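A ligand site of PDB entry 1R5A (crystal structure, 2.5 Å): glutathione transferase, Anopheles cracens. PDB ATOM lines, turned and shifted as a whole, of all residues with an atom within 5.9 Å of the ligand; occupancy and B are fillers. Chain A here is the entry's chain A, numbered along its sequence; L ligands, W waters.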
ATOM      1  N   LEU A   8       6.865  -9.277 -11.888  1.00  0.00           N
ATOM      2  CA  LEU A   8       7.661 -10.102 -10.992  1.00  0.00           C
ATOM      3  C   LEU A   8       8.849  -9.232 -10.646  1.00  0.00           C
ATOM      4  O   LEU A   8       9.642  -8.876 -11.517  1.00  0.00           O
ATOM      5  CB  LEU A   8       8.153 -11.358 -11.688  1.00  0.00           C
ATOM      6  CG  LEU A   8       8.911 -12.240 -10.699  1.00  0.00           C
ATOM      7  CD1 LEU A   8       7.886 -12.927  -9.822  1.00  0.00           C
ATOM      8  CD2 LEU A   8       9.781 -13.244 -11.435  1.00  0.00           C
ATOM      9  N   ALA A  10      11.931  -9.533  -9.535  1.00  0.00           N
ATOM     10  CA  ALA A  10      13.235  -9.879 -10.104  1.00  0.00           C
ATOM     11  C   ALA A  10      13.369  -9.665 -11.608  1.00  0.00           C
ATOM     12  O   ALA A  10      14.463  -9.396 -12.108  1.00  0.00           O
ATOM     13  CB  ALA A  10      13.570 -11.313  -9.750  1.00  0.00           C
ATOM     14  N   SER A  11      12.265  -9.780 -12.330  1.00  0.00           N
ATOM     15  CA  SER A  11      12.263  -9.628 -13.783  1.00  0.00           C
ATOM     16  C   SER A  11      12.850  -8.327 -14.335  1.00  0.00           C
ATOM     17  O   SER A  11      12.365  -7.239 -14.029  1.00  0.00           O
ATOM     18  CB  SER A  11      10.841  -9.813 -14.315  1.00  0.00           C
ATOM     19  OG  SER A  11      10.750  -9.396 -15.665  1.00  0.00           O
ATOM     20  N   PRO A  12      13.892  -8.427 -15.174  1.00  0.00           N
ATOM     21  CA  PRO A  12      14.530  -7.238 -15.758  1.00  0.00           C
ATOM     22  C   PRO A  12      13.559  -6.342 -16.530  1.00  0.00           C
ATOM     23  O   PRO A  12      13.594  -5.119 -16.385  1.00  0.00           O
ATOM     24  CB  PRO A  12      15.618  -7.840 -16.645  1.00  0.00           C
ATOM     25  CG  PRO A  12      16.005  -9.068 -15.902  1.00  0.00           C
ATOM     26  CD  PRO A  12      14.656  -9.641 -15.507  1.00  0.00           C
ATOM     27  N   PRO A  13      12.696  -6.928 -17.380  1.00  0.00           N
ATOM     28  CA  PRO A  13      11.722  -6.145 -18.156  1.00  0.00           C
ATOM     29  C   PRO A  13      10.748  -5.409 -17.235  1.00  0.00           C
ATOM     30  O   PRO A  13      10.355  -4.273 -17.512  1.00  0.00           O
ATOM     31  CB  PRO A  13      11.013  -7.200 -18.993  1.00  0.00           C
ATOM     32  CG  PRO A  13      12.038  -8.259 -19.172  1.00  0.00           C
ATOM     33  CD  PRO A  13      12.665  -8.333 -17.785  1.00  0.00           C
ATOM     34  N   CYS A  14      10.346  -6.053 -16.139  1.00  0.00           N
ATOM     35  CA  CYS A  14       9.409  -5.444 -15.210  1.00  0.00           C
ATOM     36  C   CYS A  14      10.047  -4.264 -14.491  1.00  0.00           C
ATOM     37  O   CYS A  14       9.391  -3.259 -14.233  1.00  0.00           O
ATOM     38  CB  CYS A  14       8.892  -6.480 -14.202  1.00  0.00           C
ATOM     39  SG  CYS A  14       7.705  -7.665 -14.930  1.00  0.00           S
ATOM     40  N   ILE A  35       5.673 -16.521 -12.320  1.00  0.00           N
ATOM     41  CA  ILE A  35       5.900 -17.273 -13.533  1.00  0.00           C
ATOM     42  C   ILE A  35       6.520 -18.633 -13.238  1.00  0.00           C
ATOM     43  O   ILE A  35       6.335 -19.602 -13.983  1.00  0.00           O
ATOM     44  CB  ILE A  35       6.773 -16.451 -14.461  1.00  0.00           C
ATOM     45  CG1 ILE A  35       5.960 -15.223 -14.871  1.00  0.00           C
ATOM     46  CG2 ILE A  35       7.257 -17.280 -15.645  1.00  0.00           C
ATOM     47  CD1 ILE A  35       6.643 -14.302 -15.789  1.00  0.00           C
ATOM     48  N   GLN A  40       1.094 -17.262 -14.964  1.00  0.00           N
ATOM     49  CA  GLN A  40       0.810 -16.574 -16.203  1.00  0.00           C
ATOM     50  C   GLN A  40       0.077 -17.465 -17.212  1.00  0.00           C
ATOM     51  O   GLN A  40      -0.498 -16.972 -18.184  1.00  0.00           O
ATOM     52  CB  GLN A  40       2.087 -16.040 -16.837  1.00  0.00           C
ATOM     53  CG  GLN A  40       2.878 -17.043 -17.664  1.00  0.00           C
ATOM     54  CD  GLN A  40       3.649 -18.051 -16.838  1.00  0.00           C
ATOM     55  OE1 GLN A  40       4.724 -18.493 -17.244  1.00  0.00           O
ATOM     56  NE2 GLN A  40       3.114 -18.411 -15.682  1.00  0.00           N
ATOM     57  N   LEU A  41       0.099 -18.778 -16.980  1.00  0.00           N
ATOM     58  CA  LEU A  41      -0.543 -19.718 -17.884  1.00  0.00           C
ATOM     59  C   LEU A  41      -2.041 -19.885 -17.648  1.00  0.00           C
ATOM     60  O   LEU A  41      -2.731 -20.509 -18.452  1.00  0.00           O
ATOM     61  CB  LEU A  41       0.140 -21.076 -17.830  1.00  0.00           C
ATOM     62  CG  LEU A  41       1.656 -21.091 -18.105  1.00  0.00           C
ATOM     63  CD1 LEU A  41       2.082 -22.524 -18.350  1.00  0.00           C
ATOM     64  CD2 LEU A  41       1.994 -20.242 -19.324  1.00  0.00           C
ATOM     65  N   GLN A  51       0.450 -14.063 -25.593  1.00  0.00           N
ATOM     66  CA  GLN A  51       1.818 -14.475 -25.325  1.00  0.00           C
ATOM     67  C   GLN A  51       2.068 -14.685 -23.815  1.00  0.00           C
ATOM     68  O   GLN A  51       3.166 -15.037 -23.405  1.00  0.00           O
ATOM     69  CB  GLN A  51       2.775 -13.424 -25.916  1.00  0.00           C
ATOM     70  CG  GLN A  51       4.256 -13.776 -25.860  1.00  0.00           C
ATOM     71  CD  GLN A  51       5.116 -12.928 -26.801  1.00  0.00           C
ATOM     72  OE1 GLN A  51       6.343 -13.024 -26.775  1.00  0.00           O
ATOM     73  NE2 GLN A  51       4.479 -12.113 -27.653  1.00  0.00           N
ATOM     74  N   HIS A  52       1.034 -14.482 -22.993  1.00  0.00           N
ATOM     75  CA  HIS A  52       1.134 -14.655 -21.537  1.00  0.00           C
ATOM     76  C   HIS A  52       2.486 -14.341 -20.894  1.00  0.00           C
ATOM     77  O   HIS A  52       3.111 -15.209 -20.259  1.00  0.00           O
ATOM     78  CB  HIS A  52       0.667 -16.076 -21.146  1.00  0.00           C
ATOM     79  CG  HIS A  52       1.466 -17.183 -21.766  1.00  0.00           C
ATOM     80  ND1 HIS A  52       2.744 -17.496 -21.366  1.00  0.00           N
ATOM     81  CD2 HIS A  52       1.168 -18.036 -22.781  1.00  0.00           C
ATOM     82  CE1 HIS A  52       3.212 -18.490 -22.108  1.00  0.00           C
ATOM     83  NE2 HIS A  52       2.280 -18.833 -22.974  1.00  0.00           N
ATOM     84  N   CYS A  53       2.938 -13.096 -21.024  1.00  0.00           N
ATOM     85  CA  CYS A  53       4.217 -12.698 -20.446  1.00  0.00           C
ATOM     86  C   CYS A  53       4.109 -11.409 -19.636  1.00  0.00           C
ATOM     87  O   CYS A  53       3.102 -10.701 -19.686  1.00  0.00           O
ATOM     88  CB  CYS A  53       5.253 -12.488 -21.555  1.00  0.00           C
ATOM     89  SG  CYS A  53       4.777 -11.248 -22.802  1.00  0.00           S
ATOM     90  N   ILE A  54       5.158 -11.129 -18.875  1.00  0.00           N
ATOM     91  CA  ILE A  54       5.196  -9.915 -18.078  1.00  0.00           C
ATOM     92  C   ILE A  54       6.490  -9.174 -18.393  1.00  0.00           C
ATOM     93  O   ILE A  54       7.514  -9.788 -18.709  1.00  0.00           O
ATOM     94  CB  ILE A  54       5.153 -10.230 -16.586  1.00  0.00           C
ATOM     95  CG1 ILE A  54       6.332 -11.133 -16.200  1.00  0.00           C
ATOM     96  CG2 ILE A  54       3.817 -10.858 -16.258  1.00  0.00           C
ATOM     97  CD1 ILE A  54       6.461 -11.390 -14.719  1.00  0.00           C
ATOM     98  N   PRO A  55       6.484  -7.838 -18.245  1.00  0.00           N
ATOM     99  CA  PRO A  55       5.322  -7.069 -17.801  1.00  0.00           C
ATOM    100  C   PRO A  55       4.157  -6.942 -18.769  1.00  0.00           C
ATOM    101  O   PRO A  55       4.326  -6.936 -19.989  1.00  0.00           O
ATOM    102  CB  PRO A  55       5.926  -5.711 -17.484  1.00  0.00           C
ATOM    103  CG  PRO A  55       6.934  -5.557 -18.580  1.00  0.00           C
ATOM    104  CD  PRO A  55       7.590  -6.934 -18.614  1.00  0.00           C
ATOM    105  N   TRP A  65       1.752  -5.062 -23.724  1.00  0.00           N
ATOM    106  CA  TRP A  65       2.907  -5.764 -23.151  1.00  0.00           C
ATOM    107  C   TRP A  65       4.168  -5.461 -23.981  1.00  0.00           C
ATOM    108  O   TRP A  65       4.070  -4.931 -25.098  1.00  0.00           O
ATOM    109  CB  TRP A  65       2.639  -7.285 -23.001  1.00  0.00           C
ATOM    110  CG  TRP A  65       2.356  -8.081 -24.259  1.00  0.00           C
ATOM    111  CD1 TRP A  65       3.257  -8.752 -25.035  1.00  0.00           C
ATOM    112  CD2 TRP A  65       1.074  -8.263 -24.900  1.00  0.00           C
ATOM    113  NE1 TRP A  65       2.626  -9.344 -26.101  1.00  0.00           N
ATOM    114  CE2 TRP A  65       1.286  -9.052 -26.050  1.00  0.00           C
ATOM    115  CE3 TRP A  65      -0.232  -7.826 -24.597  1.00  0.00           C
ATOM    116  CZ2 TRP A  65       0.245  -9.424 -26.916  1.00  0.00           C
ATOM    117  CZ3 TRP A  65      -1.272  -8.198 -25.463  1.00  0.00           C
ATOM    118  CH2 TRP A  65      -1.025  -8.992 -26.602  1.00  0.00           C
ATOM    119  N   GLU A  66       5.322  -5.787 -23.421  1.00  0.00           N
ATOM    120  CA  GLU A  66       6.649  -5.547 -24.006  1.00  0.00           C
ATOM    121  C   GLU A  66       7.198  -4.342 -23.270  1.00  0.00           C
ATOM    122  O   GLU A  66       6.891  -3.202 -23.596  1.00  0.00           O
ATOM    123  CB  GLU A  66       6.589  -5.248 -25.498  1.00  0.00           C
ATOM    124  CG  GLU A  66       6.538  -6.482 -26.355  1.00  0.00           C
ATOM    125  CD  GLU A  66       7.810  -7.306 -26.253  1.00  0.00           C
ATOM    126  OE1 GLU A  66       8.849  -6.755 -25.840  1.00  0.00           O
ATOM    127  OE2 GLU A  66       7.783  -8.506 -26.610  1.00  0.00           O
ATOM    128  N   SER A  67       7.992  -4.616 -22.238  1.00  0.00           N
ATOM    129  CA  SER A  67       8.562  -3.572 -21.412  1.00  0.00           C
ATOM    130  C   SER A  67       8.910  -2.262 -22.139  1.00  0.00           C
ATOM    131  O   SER A  67       8.490  -1.190 -21.711  1.00  0.00           O
ATOM    132  CB  SER A  67       9.793  -4.103 -20.658  1.00  0.00           C
ATOM    133  OG  SER A  67      10.803  -4.586 -21.543  1.00  0.00           O
ATOM    134  N   ARG A  68       9.648  -2.358 -23.243  1.00  0.00           N
ATOM    135  CA  ARG A  68      10.043  -1.148 -23.953  1.00  0.00           C
ATOM    136  C   ARG A  68       8.901  -0.403 -24.629  1.00  0.00           C
ATOM    137  O   ARG A  68       8.978   0.815 -24.833  1.00  0.00           O
ATOM    138  CB  ARG A  68      11.167  -1.474 -24.947  1.00  0.00           C
ATOM    139  CG  ARG A  68      12.341  -2.170 -24.253  1.00  0.00           C
ATOM    140  CD  ARG A  68      13.402  -2.668 -25.218  1.00  0.00           C
ATOM    141  NE  ARG A  68      14.308  -3.591 -24.555  1.00  0.00           N
ATOM    142  CZ  ARG A  68      14.058  -4.890 -24.348  1.00  0.00           C
ATOM    143  NH1 ARG A  68      12.907  -5.416 -24.775  1.00  0.00           N
ATOM    144  NH2 ARG A  68      14.941  -5.649 -23.716  1.00  0.00           N
ATOM    145  N   LEU A 103      16.544  -4.846 -26.986  1.00  0.00           N
ATOM    146  CA  LEU A 103      15.646  -5.973 -27.101  1.00  0.00           C
ATOM    147  C   LEU A 103      16.173  -7.073 -28.017  1.00  0.00           C
ATOM    148  O   LEU A 103      16.254  -8.247 -27.612  1.00  0.00           O
ATOM    149  CB  LEU A 103      14.270  -5.525 -27.602  1.00  0.00           C
ATOM    150  CG  LEU A 103      13.273  -6.658 -27.909  1.00  0.00           C
ATOM    151  CD1 LEU A 103      13.131  -7.547 -26.684  1.00  0.00           C
ATOM    152  CD2 LEU A 103      11.920  -6.093 -28.316  1.00  0.00           C
ATOM    153  N   TYR A 107      20.257  -7.445 -24.651  1.00  0.00           N
ATOM    154  CA  TYR A 107      19.518  -8.245 -23.682  1.00  0.00           C
ATOM    155  C   TYR A 107      19.316  -9.689 -24.137  1.00  0.00           C
ATOM    156  O   TYR A 107      19.454 -10.620 -23.335  1.00  0.00           O
ATOM    157  CB  TYR A 107      18.159  -7.624 -23.391  1.00  0.00           C
ATOM    158  CG  TYR A 107      17.469  -8.288 -22.239  1.00  0.00           C
ATOM    159  CD1 TYR A 107      17.965  -8.132 -20.948  1.00  0.00           C
ATOM    160  CD2 TYR A 107      16.387  -9.142 -22.424  1.00  0.00           C
ATOM    161  CE1 TYR A 107      17.410  -8.805 -19.873  1.00  0.00           C
ATOM    162  CE2 TYR A 107      15.819  -9.833 -21.358  1.00  0.00           C
ATOM    163  CZ  TYR A 107      16.347  -9.651 -20.079  1.00  0.00           C
ATOM    164  OH  TYR A 107      15.815 -10.302 -19.005  1.00  0.00           O
ATOM    165  N   PHE A 115      20.169 -17.193 -18.568  1.00  0.00           N
ATOM    166  CA  PHE A 115      18.929 -17.835 -18.138  1.00  0.00           C
ATOM    167  C   PHE A 115      18.836 -19.357 -18.226  1.00  0.00           C
ATOM    168  O   PHE A 115      18.140 -19.971 -17.417  1.00  0.00           O
ATOM    169  CB  PHE A 115      17.741 -17.181 -18.859  1.00  0.00           C
ATOM    170  CG  PHE A 115      17.462 -15.775 -18.399  1.00  0.00           C
ATOM    171  CD1 PHE A 115      16.170 -15.257 -18.462  1.00  0.00           C
ATOM    172  CD2 PHE A 115      18.484 -14.972 -17.901  1.00  0.00           C
ATOM    173  CE1 PHE A 115      15.898 -13.960 -18.026  1.00  0.00           C
ATOM    174  CE2 PHE A 115      18.226 -13.679 -17.464  1.00  0.00           C
ATOM    175  CZ  PHE A 115      16.928 -13.175 -17.526  1.00  0.00           C
ATOM    176  N   HIS A 119      17.627 -21.462 -15.479  1.00  0.00           N
ATOM    177  CA  HIS A 119      16.351 -22.159 -15.597  1.00  0.00           C
ATOM    178  C   HIS A 119      16.475 -23.668 -15.532  1.00  0.00           C
ATOM    179  O   HIS A 119      15.573 -24.346 -15.044  1.00  0.00           O
ATOM    180  CB  HIS A 119      15.655 -21.746 -16.897  1.00  0.00           C
ATOM    181  CG  HIS A 119      15.093 -20.359 -16.881  1.00  0.00           C
ATOM    182  ND1 HIS A 119      14.563 -19.756 -18.009  1.00  0.00           N
ATOM    183  CD2 HIS A 119      14.949 -19.460 -15.877  1.00  0.00           C
ATOM    184  CE1 HIS A 119      14.122 -18.547 -17.690  1.00  0.00           C
ATOM    185  NE2 HIS A 119      14.345 -18.353 -16.406  1.00  0.00           N
HETATM  186  N1  LIG L   1      10.433  -8.727 -24.450  1.00  0.00           N
HETATM  187  C1  LIG L   1       9.620  -8.915 -23.259  1.00  0.00           C
HETATM  188  C2  LIG L   1       9.680  -7.565 -22.550  1.00  0.00           C
HETATM  189  O1  LIG L   1       8.803  -7.322 -21.727  1.00  0.00           O
HETATM  190  O2  LIG L   1      10.577  -6.751 -22.806  1.00  0.00           O
HETATM  191  C3  LIG L   1      10.227 -10.046 -22.447  1.00  0.00           C
HETATM  192  C4  LIG L   1       9.436 -10.350 -21.159  1.00  0.00           C
HETATM  193  C5  LIG L   1       9.738 -11.731 -20.608  1.00  0.00           C
HETATM  194  O3  LIG L   1      10.530 -12.494 -21.169  1.00  0.00           O
HETATM  195  N2  LIG L   1       9.071 -12.023 -19.498  1.00  0.00           N
HETATM  196  C6  LIG L   1       9.221 -13.312 -18.825  1.00  0.00           C
HETATM  197  C7  LIG L   1       7.885 -13.971 -18.795  1.00  0.00           C
HETATM  198  O4  LIG L   1       6.855 -13.303 -18.623  1.00  0.00           O
HETATM  199  C8  LIG L   1       9.645 -13.233 -17.370  1.00  0.00           C
HETATM  200  S1  LIG L   1      11.266 -12.536 -17.036  1.00  0.00           S
HETATM  201  O5  LIG L   1      11.383 -11.199 -17.548  1.00  0.00           O
HETATM  202  O6  LIG L   1      11.442 -12.543 -15.620  1.00  0.00           O
HETATM  203  O7  LIG L   1      12.274 -13.336 -17.672  1.00  0.00           O
HETATM  204  N3  LIG L   1       7.932 -15.300 -18.963  1.00  0.00           N
HETATM  205  C9  LIG L   1       6.770 -16.167 -18.948  1.00  0.00           C
HETATM  206  C10 LIG L   1       6.188 -16.424 -20.314  1.00  0.00           C
HETATM  207  O8  LIG L   1       5.274 -17.232 -20.349  1.00  0.00           O
HETATM  208  O9  LIG L   1       6.693 -15.857 -21.303  1.00  0.00           O
HETATM  209  O   HOH W   1       6.137  -7.936 -21.291  1.00  0.00           O
HETATM  210  O   HOH W   2      13.461  -8.670 -23.082  1.00  0.00           O
HETATM  211  O   HOH W   3      10.908 -10.943 -26.259  1.00  0.00           O
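OG of Ser 11 sits at hydrogen-bond distance from N of Cys 14.
Residues that only touch the ligand: Ile 35 (3.0 Å), Pro 13 (3.1 Å), Cys 53 (3.3 Å), Pro 55 (3.4 Å), Phe 115 (3.7 Å) and Leu 103 (3.7 Å).
Hydrophobic or aromatic side chains that line the ligand: Pro 13, Ile 35, His 52, Ile 54, Pro 55, Leu 103 and Phe 115.
13 residues have an atom within 4 Å of the ligand: Ser 11, Pro 13, Ile 35, Gln 40, His 52, Cys 53, Ile 54, Pro 55, Glu 66, Ser 67, Arg 68, Leu 103 and Phe 115.
The nearest printed residue that does not touch the ligand is Pro 12 (4.2 Å).
Water W1 lies within hydrogen-bond range of the backbone carbonyl oxygen (O) of Pro 55 (2.4 Å), an oxygen (O1) of the ligand (2.8 Å), the backbone NH (N) of Glu 66 (3.1 Å) and the backbone carbonyl oxygen (O) of Ile 54 (3.5 Å).
Water W2 bridges a nitrogen (N1) of the ligand (3.3 Å) and the guanidinium group of Arg 68 (3.4 Å).
The backbone NH (N) of Ile 54 lies within hydrogen-bond range of an oxygen (O4) of the ligand (2.8 Å).
OG of Ser 11 sits at hydrogen-bond distance from O5 of the ligand (2.7 Å).
The backbone carbonyl oxygen of Ile 54 lies within hydrogen-bond range of a nitrogen (N2) of the ligand.
The backbone NH (N) of Ser 67 is in hydrogen-bond range of an oxygen (O1) of the ligand.
OG of Ser 67 sits at hydrogen-bond distance from O2 of the ligand (2.5 Å).
ND1 of His 52 is in hydrogen-bond range of O8 of the ligand (2.7 Å).
OE1 of Gln 40 lies close to O8 of the ligand, 3.4 Å away.
The backbone carbonyl oxygen (O) of His 52 lies close to an oxygen (O8) of the ligand.
NH1 of Arg 68 is in salt-bridge range of O2 of the ligand (3.3 Å).
OE1 of Glu 66 is in salt-bridge range of N1 of the ligand (2.9 Å).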
